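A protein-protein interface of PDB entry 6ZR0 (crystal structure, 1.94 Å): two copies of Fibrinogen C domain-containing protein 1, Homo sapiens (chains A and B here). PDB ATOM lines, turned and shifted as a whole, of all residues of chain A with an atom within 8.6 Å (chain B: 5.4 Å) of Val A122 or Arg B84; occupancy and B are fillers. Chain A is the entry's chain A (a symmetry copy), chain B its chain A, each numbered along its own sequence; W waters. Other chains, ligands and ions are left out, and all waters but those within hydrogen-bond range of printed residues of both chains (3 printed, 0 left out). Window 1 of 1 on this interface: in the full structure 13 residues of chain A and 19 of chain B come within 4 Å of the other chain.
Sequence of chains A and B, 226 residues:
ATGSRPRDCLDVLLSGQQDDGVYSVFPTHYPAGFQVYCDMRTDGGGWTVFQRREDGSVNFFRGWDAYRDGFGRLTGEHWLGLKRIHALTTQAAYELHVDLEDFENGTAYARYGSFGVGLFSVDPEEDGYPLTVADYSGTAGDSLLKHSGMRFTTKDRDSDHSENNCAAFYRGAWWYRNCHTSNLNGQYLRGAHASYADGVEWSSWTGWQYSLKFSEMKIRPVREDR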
ATOM      1  N   HIS A  86      18.249  16.088 -33.770  1.00  0.00           N
ATOM      2  CA  HIS A  86      17.716  14.780 -33.296  1.00  0.00           C
ATOM      3  C   HIS A  86      16.841  14.147 -34.386  1.00  0.00           C
ATOM      4  O   HIS A  86      17.091  12.977 -34.733  1.00  0.00           O
ATOM      5  CB  HIS A  86      16.938  14.935 -31.983  1.00  0.00           C
ATOM      6  CG  HIS A  86      16.231  13.687 -31.576  1.00  0.00           C
ATOM      7  ND1 HIS A  86      14.908  13.448 -31.901  1.00  0.00           N
ATOM      8  CD2 HIS A  86      16.661  12.594 -30.909  1.00  0.00           C
ATOM      9  CE1 HIS A  86      14.550  12.268 -31.436  1.00  0.00           C
ATOM     10  NE2 HIS A  86      15.606  11.726 -30.821  1.00  0.00           N
ATOM     11  N   GLY A 118      20.958  12.153 -29.199  1.00  0.00           N
ATOM     12  CA  GLY A 118      19.857  11.494 -28.468  1.00  0.00           C
ATOM     13  C   GLY A 118      19.261  10.333 -29.249  1.00  0.00           C
ATOM     14  O   GLY A 118      18.022  10.190 -29.232  1.00  0.00           O
ATOM     15  N   LEU A 119      20.112   9.517 -29.884  1.00  0.00           N
ATOM     16  CA  LEU A 119      19.709   8.491 -30.888  1.00  0.00           C
ATOM     17  C   LEU A 119      18.704   7.494 -30.295  1.00  0.00           C
ATOM     18  O   LEU A 119      17.831   7.036 -31.062  1.00  0.00           O
ATOM     19  CB  LEU A 119      20.948   7.760 -31.415  1.00  0.00           C
ATOM     20  CG  LEU A 119      21.806   8.525 -32.425  1.00  0.00           C
ATOM     21  CD1 LEU A 119      22.887   7.620 -32.995  1.00  0.00           C
ATOM     22  CD2 LEU A 119      20.964   9.110 -33.551  1.00  0.00           C
ATOM     23  N   PHE A 120      18.831   7.149 -29.009  1.00  0.00           N
ATOM     24  CA  PHE A 120      18.005   6.110 -28.335  1.00  0.00           C
ATOM     25  C   PHE A 120      17.256   6.697 -27.131  1.00  0.00           C
ATOM     26  O   PHE A 120      16.632   5.917 -26.388  1.00  0.00           O
ATOM     27  CB  PHE A 120      18.887   4.927 -27.929  1.00  0.00           C
ATOM     28  CG  PHE A 120      19.619   4.282 -29.079  1.00  0.00           C
ATOM     29  CD1 PHE A 120      18.931   3.536 -30.023  1.00  0.00           C
ATOM     30  CD2 PHE A 120      20.990   4.428 -29.225  1.00  0.00           C
ATOM     31  CE1 PHE A 120      19.599   2.946 -31.086  1.00  0.00           C
ATOM     32  CE2 PHE A 120      21.656   3.836 -30.288  1.00  0.00           C
ATOM     33  CZ  PHE A 120      20.961   3.097 -31.215  1.00  0.00           C
ATOM     34  N   SER A 121      17.285   8.022 -26.959  1.00  0.00           N
ATOM     35  CA  SER A 121      16.588   8.746 -25.864  1.00  0.00           C
ATOM     36  C   SER A 121      15.077   8.714 -26.119  1.00  0.00           C
ATOM     37  O   SER A 121      14.661   9.110 -27.222  1.00  0.00           O
ATOM     38  CB  SER A 121      17.087  10.161 -25.746  1.00  0.00           C
ATOM     39  OG  SER A 121      18.500  10.193 -25.606  1.00  0.00           O
ATOM     40  N   VAL A 122      14.292   8.254 -25.139  1.00  0.00           N
ATOM     41  CA  VAL A 122      12.799   8.263 -25.191  1.00  0.00           C
ATOM     42  C   VAL A 122      12.341   9.721 -25.296  1.00  0.00           C
ATOM     43  O   VAL A 122      11.485  10.015 -26.152  1.00  0.00           O
ATOM     44  CB  VAL A 122      12.175   7.561 -23.969  1.00  0.00           C
ATOM     45  CG1 VAL A 122      10.667   7.758 -23.913  1.00  0.00           C
ATOM     46  CG2 VAL A 122      12.519   6.080 -23.935  1.00  0.00           C
ATOM     47  N   ASP A 123      12.891  10.582 -24.437  1.00  0.00           N
ATOM     48  CA  ASP A 123      12.725  12.059 -24.473  1.00  0.00           C
ATOM     49  C   ASP A 123      14.113  12.683 -24.604  1.00  0.00           C
ATOM     50  O   ASP A 123      14.797  12.888 -23.603  1.00  0.00           O
ATOM     51  CB  ASP A 123      11.963  12.552 -23.239  1.00  0.00           C
ATOM     52  CG  ASP A 123      11.639  14.037 -23.256  1.00  0.00           C
ATOM     53  OD1 ASP A 123      12.012  14.710 -24.235  1.00  0.00           O
ATOM     54  OD2 ASP A 123      11.016  14.508 -22.285  1.00  0.00           O
ATOM     55  N   PRO A 124      14.581  12.988 -25.838  1.00  0.00           N
ATOM     56  CA  PRO A 124      15.938  13.497 -26.043  1.00  0.00           C
ATOM     57  C   PRO A 124      16.227  14.810 -25.298  1.00  0.00           C
ATOM     58  O   PRO A 124      17.369  15.014 -24.925  1.00  0.00           O
ATOM     59  CB  PRO A 124      16.042  13.683 -27.567  1.00  0.00           C
ATOM     60  CG  PRO A 124      14.607  13.760 -28.041  1.00  0.00           C
ATOM     61  CD  PRO A 124      13.839  12.856 -27.102  1.00  0.00           C
ATOM     62  N   GLU A 125      15.207  15.649 -25.078  1.00  0.00           N
ATOM     63  CA  GLU A 125      15.341  16.920 -24.315  1.00  0.00           C
ATOM     64  C   GLU A 125      15.643  16.599 -22.846  1.00  0.00           C
ATOM     65  O   GLU A 125      16.645  17.126 -22.328  1.00  0.00           O
ATOM     66  CB  GLU A 125      14.086  17.788 -24.426  1.00  0.00           C
ATOM     67  CG  GLU A 125      14.288  19.174 -23.842  1.00  0.00           C
ATOM     68  CD  GLU A 125      13.061  20.065 -23.786  1.00  0.00           C
ATOM     69  OE1 GLU A 125      12.004  19.655 -24.302  1.00  0.00           O
ATOM     70  OE2 GLU A 125      13.172  21.175 -23.230  1.00  0.00           O
ATOM     71  N   GLU A 126      14.799  15.780 -22.211  1.00  0.00           N
ATOM     72  CA  GLU A 126      14.993  15.262 -20.827  1.00  0.00           C
ATOM     73  C   GLU A 126      16.405  14.674 -20.718  1.00  0.00           C
ATOM     74  O   GLU A 126      17.131  15.044 -19.775  1.00  0.00           O
ATOM     75  CB  GLU A 126      13.927  14.212 -20.496  1.00  0.00           C
ATOM     76  CG  GLU A 126      14.071  13.577 -19.119  1.00  0.00           C
ATOM     77  CD  GLU A 126      14.900  12.301 -19.042  1.00  0.00           C
ATOM     78  OE1 GLU A 126      14.947  11.550 -20.039  1.00  0.00           O
ATOM     79  OE2 GLU A 126      15.498  12.059 -17.977  1.00  0.00           O
ATOM     80  N   ASP A 127      16.778  13.829 -21.684  1.00  0.00           N
ATOM     81  CA  ASP A 127      18.037  13.037 -21.681  1.00  0.00           C
ATOM     82  C   ASP A 127      19.234  13.921 -22.063  1.00  0.00           C
ATOM     83  O   ASP A 127      20.368  13.414 -21.997  1.00  0.00           O
ATOM     84  CB  ASP A 127      17.921  11.830 -22.616  1.00  0.00           C
ATOM     85  CG  ASP A 127      18.884  10.704 -22.284  1.00  0.00           C
ATOM     86  OD1 ASP A 127      19.192  10.530 -21.089  1.00  0.00           O
ATOM     87  OD2 ASP A 127      19.322  10.013 -23.225  1.00  0.00           O
ATOM     88  N   PRO A 130      22.235  13.526 -25.858  1.00  0.00           N
ATOM     89  CA  PRO A 130      23.591  12.983 -25.753  1.00  0.00           C
ATOM     90  C   PRO A 130      24.248  12.743 -27.122  1.00  0.00           C
ATOM     91  O   PRO A 130      23.564  12.324 -28.042  1.00  0.00           O
ATOM     92  CB  PRO A 130      23.410  11.658 -24.993  1.00  0.00           C
ATOM     93  CG  PRO A 130      21.949  11.306 -25.187  1.00  0.00           C
ATOM     94  CD  PRO A 130      21.229  12.635 -25.261  1.00  0.00           C
ATOM     95  N   PRO B  27       1.403   5.507 -34.620  1.00  0.00           N
ATOM     96  CA  PRO B  27       0.038   5.254 -34.154  1.00  0.00           C
ATOM     97  C   PRO B  27      -0.999   6.174 -34.815  1.00  0.00           C
ATOM     98  O   PRO B  27      -0.647   7.274 -35.201  1.00  0.00           O
ATOM     99  CB  PRO B  27       0.110   5.510 -32.640  1.00  0.00           C
ATOM    100  CG  PRO B  27       1.572   5.308 -32.302  1.00  0.00           C
ATOM    101  CD  PRO B  27       2.316   5.832 -33.513  1.00  0.00           C
ATOM    102  N   TYR B  30      -1.168   9.591 -33.387  1.00  0.00           N
ATOM    103  CA  TYR B  30       0.209  10.093 -33.133  1.00  0.00           C
ATOM    104  C   TYR B  30       0.982  10.008 -34.450  1.00  0.00           C
ATOM    105  O   TYR B  30       1.991   9.311 -34.540  1.00  0.00           O
ATOM    106  CB  TYR B  30       0.841   9.290 -31.991  1.00  0.00           C
ATOM    107  CG  TYR B  30       1.867  10.018 -31.158  1.00  0.00           C
ATOM    108  CD1 TYR B  30       2.985  10.602 -31.733  1.00  0.00           C
ATOM    109  CD2 TYR B  30       1.745  10.081 -29.778  1.00  0.00           C
ATOM    110  CE1 TYR B  30       3.938  11.254 -30.965  1.00  0.00           C
ATOM    111  CE2 TYR B  30       2.689  10.727 -28.995  1.00  0.00           C
ATOM    112  CZ  TYR B  30       3.789  11.316 -29.591  1.00  0.00           C
ATOM    113  OH  TYR B  30       4.724  11.953 -28.827  1.00  0.00           O
ATOM    114  N   PHE B  34       7.100   7.824 -33.360  1.00  0.00           N
ATOM    115  CA  PHE B  34       8.224   7.807 -32.393  1.00  0.00           C
ATOM    116  C   PHE B  34       8.925   6.453 -32.490  1.00  0.00           C
ATOM    117  O   PHE B  34       8.372   5.531 -33.127  1.00  0.00           O
ATOM    118  CB  PHE B  34       7.715   8.080 -30.975  1.00  0.00           C
ATOM    119  CG  PHE B  34       6.502   7.274 -30.583  1.00  0.00           C
ATOM    120  CD1 PHE B  34       6.634   5.983 -30.096  1.00  0.00           C
ATOM    121  CD2 PHE B  34       5.228   7.803 -30.712  1.00  0.00           C
ATOM    122  CE1 PHE B  34       5.516   5.244 -29.737  1.00  0.00           C
ATOM    123  CE2 PHE B  34       4.113   7.063 -30.353  1.00  0.00           C
ATOM    124  CZ  PHE B  34       4.258   5.784 -29.868  1.00  0.00           C
ATOM    125  N   ARG B  68       4.382  11.042 -18.203  1.00  0.00           N
ATOM    126  CA  ARG B  68       3.587  11.415 -19.403  1.00  0.00           C
ATOM    127  C   ARG B  68       4.472  11.295 -20.650  1.00  0.00           C
ATOM    128  O   ARG B  68       4.046  10.630 -21.612  1.00  0.00           O
ATOM    129  CB  ARG B  68       3.036  12.836 -19.267  1.00  0.00           C
ATOM    130  CG  ARG B  68       2.167  13.288 -20.434  1.00  0.00           C
ATOM    131  CD  ARG B  68       1.829  14.761 -20.319  1.00  0.00           C
ATOM    132  NE  ARG B  68       3.041  15.567 -20.383  1.00  0.00           N
ATOM    133  CZ  ARG B  68       3.271  16.684 -19.697  1.00  0.00           C
ATOM    134  NH1 ARG B  68       2.367  17.170 -18.861  1.00  0.00           N
ATOM    135  NH2 ARG B  68       4.424  17.314 -19.846  1.00  0.00           N
ATOM    136  N   ASP B  69       5.656  11.916 -20.620  1.00  0.00           N
ATOM    137  CA  ASP B  69       6.503  12.175 -21.815  1.00  0.00           C
ATOM    138  C   ASP B  69       7.517  11.046 -22.021  1.00  0.00           C
ATOM    139  O   ASP B  69       7.993  10.900 -23.162  1.00  0.00           O
ATOM    140  CB  ASP B  69       7.206  13.530 -21.703  1.00  0.00           C
ATOM    141  CG  ASP B  69       6.255  14.714 -21.758  1.00  0.00           C
ATOM    142  OD1 ASP B  69       5.154  14.559 -22.329  1.00  0.00           O
ATOM    143  OD2 ASP B  69       6.615  15.779 -21.218  1.00  0.00           O
ATOM    144  N   GLY B  70       7.848  10.296 -20.965  1.00  0.00           N
ATOM    145  CA  GLY B  70       8.797   9.167 -21.018  1.00  0.00           C
ATOM    146  C   GLY B  70      10.210   9.593 -20.653  1.00  0.00           C
ATOM    147  O   GLY B  70      10.502  10.806 -20.696  1.00  0.00           O
ATOM    148  N   PHE B  71      11.061   8.628 -20.299  1.00  0.00           N
ATOM    149  CA  PHE B  71      12.462   8.856 -19.858  1.00  0.00           C
ATOM    150  C   PHE B  71      13.277   7.573 -20.053  1.00  0.00           C
ATOM    151  O   PHE B  71      12.682   6.518 -20.348  1.00  0.00           O
ATOM    152  CB  PHE B  71      12.489   9.335 -18.403  1.00  0.00           C
ATOM    153  CG  PHE B  71      11.818   8.415 -17.415  1.00  0.00           C
ATOM    154  CD1 PHE B  71      12.522   7.383 -16.812  1.00  0.00           C
ATOM    155  CD2 PHE B  71      10.484   8.586 -17.078  1.00  0.00           C
ATOM    156  CE1 PHE B  71      11.904   6.539 -15.903  1.00  0.00           C
ATOM    157  CE2 PHE B  71       9.869   7.745 -16.163  1.00  0.00           C
ATOM    158  CZ  PHE B  71      10.580   6.724 -15.577  1.00  0.00           C
ATOM    159  N   GLY B  72      14.598   7.676 -19.880  1.00  0.00           N
ATOM    160  CA  GLY B  72      15.555   6.576 -20.099  1.00  0.00           C
ATOM    161  C   GLY B  72      15.857   6.397 -21.575  1.00  0.00           C
ATOM    162  O   GLY B  72      15.550   7.319 -22.360  1.00  0.00           O
ATOM    163  N   ARG B  73      16.431   5.250 -21.946  1.00  0.00           N
ATOM    164  CA  ARG B  73      16.856   4.944 -23.337  1.00  0.00           C
ATOM    165  C   ARG B  73      16.246   3.608 -23.772  1.00  0.00           C
ATOM    166  O   ARG B  73      16.156   2.688 -22.931  1.00  0.00           O
ATOM    167  CB  ARG B  73      18.384   4.970 -23.433  1.00  0.00           C
ATOM    168  CG  ARG B  73      18.952   6.381 -23.387  1.00  0.00           C
ATOM    169  CD  ARG B  73      20.460   6.452 -23.257  1.00  0.00           C
ATOM    170  NE  ARG B  73      20.865   7.761 -22.763  1.00  0.00           N
ATOM    171  CZ  ARG B  73      22.100   8.100 -22.400  1.00  0.00           C
ATOM    172  NH1 ARG B  73      23.089   7.222 -22.475  1.00  0.00           N
ATOM    173  NH2 ARG B  73      22.341   9.323 -21.960  1.00  0.00           N
ATOM    174  N   LEU B  74      15.850   3.523 -25.045  1.00  0.00           N
ATOM    175  CA  LEU B  74      15.095   2.385 -25.636  1.00  0.00           C
ATOM    176  C   LEU B  74      15.938   1.104 -25.575  1.00  0.00           C
ATOM    177  O   LEU B  74      15.340   0.012 -25.507  1.00  0.00           O
ATOM    178  CB  LEU B  74      14.721   2.734 -27.082  1.00  0.00           C
ATOM    179  CG  LEU B  74      13.745   3.899 -27.247  1.00  0.00           C
ATOM    180  CD1 LEU B  74      13.662   4.337 -28.701  1.00  0.00           C
ATOM    181  CD2 LEU B  74      12.366   3.534 -26.722  1.00  0.00           C
ATOM    182  N   HIS B  78      14.009   2.178 -19.378  1.00  0.00           N
ATOM    183  CA  HIS B  78      13.185   3.302 -19.887  1.00  0.00           C
ATOM    184  C   HIS B  78      11.714   3.125 -19.511  1.00  0.00           C
ATOM    185  O   HIS B  78      11.308   2.011 -19.117  1.00  0.00           O
ATOM    186  CB  HIS B  78      13.367   3.468 -21.402  1.00  0.00           C
ATOM    187  CG  HIS B  78      12.758   2.386 -22.230  1.00  0.00           C
ATOM    188  ND1 HIS B  78      13.392   1.180 -22.457  1.00  0.00           N
ATOM    189  CD2 HIS B  78      11.589   2.334 -22.906  1.00  0.00           C
ATOM    190  CE1 HIS B  78      12.635   0.426 -23.230  1.00  0.00           C
ATOM    191  NE2 HIS B  78      11.522   1.113 -23.522  1.00  0.00           N
ATOM    192  N   TRP B  79      10.978   4.231 -19.608  1.00  0.00           N
ATOM    193  CA  TRP B  79       9.499   4.314 -19.594  1.00  0.00           C
ATOM    194  C   TRP B  79       9.077   5.084 -20.845  1.00  0.00           C
ATOM    195  O   TRP B  79       9.507   6.243 -20.979  1.00  0.00           O
ATOM    196  CB  TRP B  79       9.017   4.995 -18.309  1.00  0.00           C
ATOM    197  CG  TRP B  79       7.535   5.189 -18.260  1.00  0.00           C
ATOM    198  CD1 TRP B  79       6.839   6.315 -18.586  1.00  0.00           C
ATOM    199  CD2 TRP B  79       6.559   4.208 -17.874  1.00  0.00           C
ATOM    200  NE1 TRP B  79       5.497   6.103 -18.427  1.00  0.00           N
ATOM    201  CE2 TRP B  79       5.294   4.821 -17.989  1.00  0.00           C
ATOM    202  CE3 TRP B  79       6.629   2.879 -17.441  1.00  0.00           C
ATOM    203  CZ2 TRP B  79       4.112   4.149 -17.682  1.00  0.00           C
ATOM    204  CZ3 TRP B  79       5.461   2.216 -17.139  1.00  0.00           C
ATOM    205  CH2 TRP B  79       4.220   2.843 -17.262  1.00  0.00           C
ATOM    206  N   LEU B  80       8.304   4.459 -21.737  1.00  0.00           N
ATOM    207  CA  LEU B  80       8.001   5.006 -23.087  1.00  0.00           C
ATOM    208  C   LEU B  80       7.201   6.307 -22.954  1.00  0.00           C
ATOM    209  O   LEU B  80       7.343   7.167 -23.835  1.00  0.00           O
ATOM    210  CB  LEU B  80       7.240   3.960 -23.908  1.00  0.00           C
ATOM    211  CG  LEU B  80       6.946   4.338 -25.361  1.00  0.00           C
ATOM    212  CD1 LEU B  80       8.233   4.560 -26.143  1.00  0.00           C
ATOM    213  CD2 LEU B  80       6.093   3.273 -26.033  1.00  0.00           C
ATOM    214  N   GLY B  81       6.405   6.439 -21.887  1.00  0.00           N
ATOM    215  CA  GLY B  81       5.552   7.614 -21.623  1.00  0.00           C
ATOM    216  C   GLY B  81       4.090   7.284 -21.854  1.00  0.00           C
ATOM    217  O   GLY B  81       3.785   6.635 -22.873  1.00  0.00           O
ATOM    218  N   LEU B  82       3.213   7.720 -20.946  1.00  0.00           N
ATOM    219  CA  LEU B  82       1.767   7.369 -20.943  1.00  0.00           C
ATOM    220  C   LEU B  82       1.068   7.942 -22.182  1.00  0.00           C
ATOM    221  O   LEU B  82       0.114   7.297 -22.658  1.00  0.00           O
ATOM    222  CB  LEU B  82       1.128   7.874 -19.646  1.00  0.00           C
ATOM    223  CG  LEU B  82       1.476   7.051 -18.406  1.00  0.00           C
ATOM    224  CD1 LEU B  82       1.219   7.842 -17.134  1.00  0.00           C
ATOM    225  CD2 LEU B  82       0.702   5.739 -18.386  1.00  0.00           C
ATOM    226  N   LYS B  83       1.518   9.090 -22.700  1.00  0.00           N
ATOM    227  CA  LYS B  83       0.941   9.694 -23.934  1.00  0.00           C
ATOM    228  C   LYS B  83       1.132   8.712 -25.100  1.00  0.00           C
ATOM    229  O   LYS B  83       0.178   8.533 -25.880  1.00  0.00           O
ATOM    230  CB  LYS B  83       1.544  11.076 -24.208  1.00  0.00           C
ATOM    231  CG  LYS B  83       2.976  11.094 -24.726  1.00  0.00           C
ATOM    232  CD  LYS B  83       3.573  12.485 -24.765  1.00  0.00           C
ATOM    233  CE  LYS B  83       4.968  12.524 -25.348  1.00  0.00           C
ATOM    234  NZ  LYS B  83       5.503  13.906 -25.370  1.00  0.00           N
ATOM    235  N   ARG B  84       2.301   8.069 -25.185  1.00  0.00           N
ATOM    236  CA  ARG B  84       2.638   7.074 -26.242  1.00  0.00           C
ATOM    237  C   ARG B  84       1.882   5.761 -25.997  1.00  0.00           C
ATOM    238  O   ARG B  84       1.379   5.185 -26.980  1.00  0.00           O
ATOM    239  CB  ARG B  84       4.150   6.833 -26.291  1.00  0.00           C
ATOM    240  CG  ARG B  84       4.936   8.039 -26.782  1.00  0.00           C
ATOM    241  CD  ARG B  84       6.407   7.739 -26.975  1.00  0.00           C
ATOM    242  NE  ARG B  84       7.121   8.918 -27.447  1.00  0.00           N
ATOM    243  CZ  ARG B  84       7.537   9.917 -26.676  1.00  0.00           C
ATOM    244  NH1 ARG B  84       7.321   9.898 -25.371  1.00  0.00           N
ATOM    245  NH2 ARG B  84       8.175  10.940 -27.219  1.00  0.00           N
ATOM    246  N   ILE B  85       1.812   5.301 -24.743  1.00  0.00           N
ATOM    247  CA  ILE B  85       1.129   4.026 -24.368  1.00  0.00           C
ATOM    248  C   ILE B  85      -0.368   4.178 -24.679  1.00  0.00           C
ATOM    249  O   ILE B  85      -0.961   3.214 -25.202  1.00  0.00           O
ATOM    250  CB  ILE B  85       1.402   3.647 -22.896  1.00  0.00           C
ATOM    251  CG1 ILE B  85       2.899   3.457 -22.625  1.00  0.00           C
ATOM    252  CG2 ILE B  85       0.611   2.406 -22.502  1.00  0.00           C
ATOM    253  CD1 ILE B  85       3.286   3.595 -21.170  1.00  0.00           C
ATOM    254  N   HIS B  86      -0.945   5.352 -24.396  1.00  0.00           N
ATOM    255  CA  HIS B  86      -2.344   5.713 -24.755  1.00  0.00           C
ATOM    256  C   HIS B  86      -2.532   5.627 -26.276  1.00  0.00           C
ATOM    257  O   HIS B  86      -3.477   4.943 -26.713  1.00  0.00           O
ATOM    258  CB  HIS B  86      -2.715   7.107 -24.230  1.00  0.00           C
ATOM    259  CG  HIS B  86      -4.038   7.582 -24.729  1.00  0.00           C
ATOM    260  ND1 HIS B  86      -4.161   8.378 -25.853  1.00  0.00           N
ATOM    261  CD2 HIS B  86      -5.294   7.348 -24.291  1.00  0.00           C
ATOM    262  CE1 HIS B  86      -5.435   8.628 -26.074  1.00  0.00           C
ATOM    263  NE2 HIS B  86      -6.151   8.011 -25.128  1.00  0.00           N
ATOM    264  N   ALA B  87      -1.673   6.306 -27.045  1.00  0.00           N
ATOM    265  CA  ALA B  87      -1.723   6.366 -28.527  1.00  0.00           C
ATOM    266  C   ALA B  87      -1.693   4.945 -29.106  1.00  0.00           C
ATOM    267  O   ALA B  87      -2.447   4.674 -30.065  1.00  0.00           O
ATOM    268  CB  ALA B  87      -0.579   7.194 -29.057  1.00  0.00           C
ATOM    269  N   LEU B  88      -0.856   4.072 -28.539  1.00  0.00           N
ATOM    270  CA  LEU B  88      -0.698   2.664 -28.991  1.00  0.00           C
ATOM    271  C   LEU B  88      -1.963   1.861 -28.660  1.00  0.00           C
ATOM    272  O   LEU B  88      -2.536   1.275 -29.591  1.00  0.00           O
ATOM    273  CB  LEU B  88       0.547   2.053 -28.337  1.00  0.00           C
ATOM    274  CG  LEU B  88       1.881   2.519 -28.920  1.00  0.00           C
ATOM    275  CD1 LEU B  88       3.037   2.146 -28.007  1.00  0.00           C
ATOM    276  CD2 LEU B  88       2.096   1.950 -30.316  1.00  0.00           C
ATOM    277  N   THR B  89      -2.397   1.853 -27.396  1.00  0.00           N
ATOM    278  CA  THR B  89      -3.405   0.890 -26.870  1.00  0.00           C
ATOM    279  C   THR B  89      -4.835   1.276 -27.285  1.00  0.00           C
ATOM    280  O   THR B  89      -5.724   0.417 -27.130  1.00  0.00           O
ATOM    281  CB  THR B  89      -3.282   0.725 -25.349  1.00  0.00           C
ATOM    282  OG1 THR B  89      -3.471   1.989 -24.712  1.00  0.00           O
ATOM    283  CG2 THR B  89      -1.950   0.139 -24.933  1.00  0.00           C
HETATM  284  O   HOH W   1      14.907  10.010 -22.446  1.00  0.00           O
HETATM  285  O   HOH W   2      16.095   9.384 -18.025  1.00  0.00           O
HETATM  286  O   HOH W   3      10.359  13.328 -19.986  1.00  0.00           O
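O of Gly B72 touches CA of Ser A121, 3.9 Å away. Val A122 touches Gly B70 (CG1 to CA, 3.7 Å). CG2 of Val A122 touches O of Phe B71 (3.6 Å). Leu B74 touches Val A122 (CD2 to CG2, 3.8 Å). His B78 touches Val A122. Val A122 touches Trp B79. CG1 of Val A122 touches O of Leu B80, 3.4 Å away. CB of Asp B69 touches OD2 of Asp A123, at 3.98 Å. Gly B70 touches Asp A123 (O to CB, 3.4 Å). Glu A126 touches Phe B71 (OE1 to CA, 3.7 Å).
Of the printed residues of chain B, Phe A120 touches Arg B73 (3.2 Å) and Leu B74 (2.9 Å). Val A122 touches eight residues of chain B. Printed residues of chain B within 4 Å of Asp A127: Arg B73. Gly B70 touches just these residues of chain A: Val A122 (3.7 Å) and Asp A123 (3.4 Å). Printed residues of chain A within 4 Å of His B78: Val A122 (3.7 Å). Arg B84 touches one residue of chain A. His B86 touches none of the printed residues of chain A. The nearest residue of chain B that does not touch Val A122 is Asp B69 (4.2 Å).
Water W3 bridges O of Gly B70 (2.6 Å) and OD2 of Asp A123 (2.7 Å). Water W2 lies within hydrogen-bond range of the side-chain carboxylate of Glu A126 (2.7 Å) and the backbone NH of Gly B72 (2.9 Å). Water W1 lies within hydrogen-bond range of the backbone carbonyl oxygen of Gly B72 (2.8 Å), the side-chain carboxylate of Glu A126 (2.9 Å), the backbone NH of Asp A123 (2.9 Å) and the backbone NH of Val A122 (3.3 Å).
N of Glu A125 lies close to OD1 of Asp A123 (3.4 Å). OD2 of Asp A127 lies within hydrogen-bond range of OG of Ser A121. O of Arg B73 sits at hydrogen-bond distance from ND1 of His B78 (3.2 Å). N of Phe B71 lies within hydrogen-bond range of O of Trp B79 (2.9 Å). The side-chain carboxylate (OD1) of Asp B69 is in salt-bridge range of the side-chain amino group (NZ) of Lys B83. The backbone carbonyl oxygen of Leu B80 lies within hydrogen-bond range of the guanidinium group of Arg B84 (3.1 Å).
Position printed for both chains: 86.
Of the 22 printed residues of chain B, 10 touch a printed residue of chain A.
O of Gly B72 lies within hydrogen-bond range of N of Val A122 (3.2 Å). The side-chain carboxylate (OD2) of Asp A127 is in salt-bridge range of the guanidinium group (NE) of Arg B73. N of Leu B74 sits at hydrogen-bond distance from O of Phe A120 (2.9 Å).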
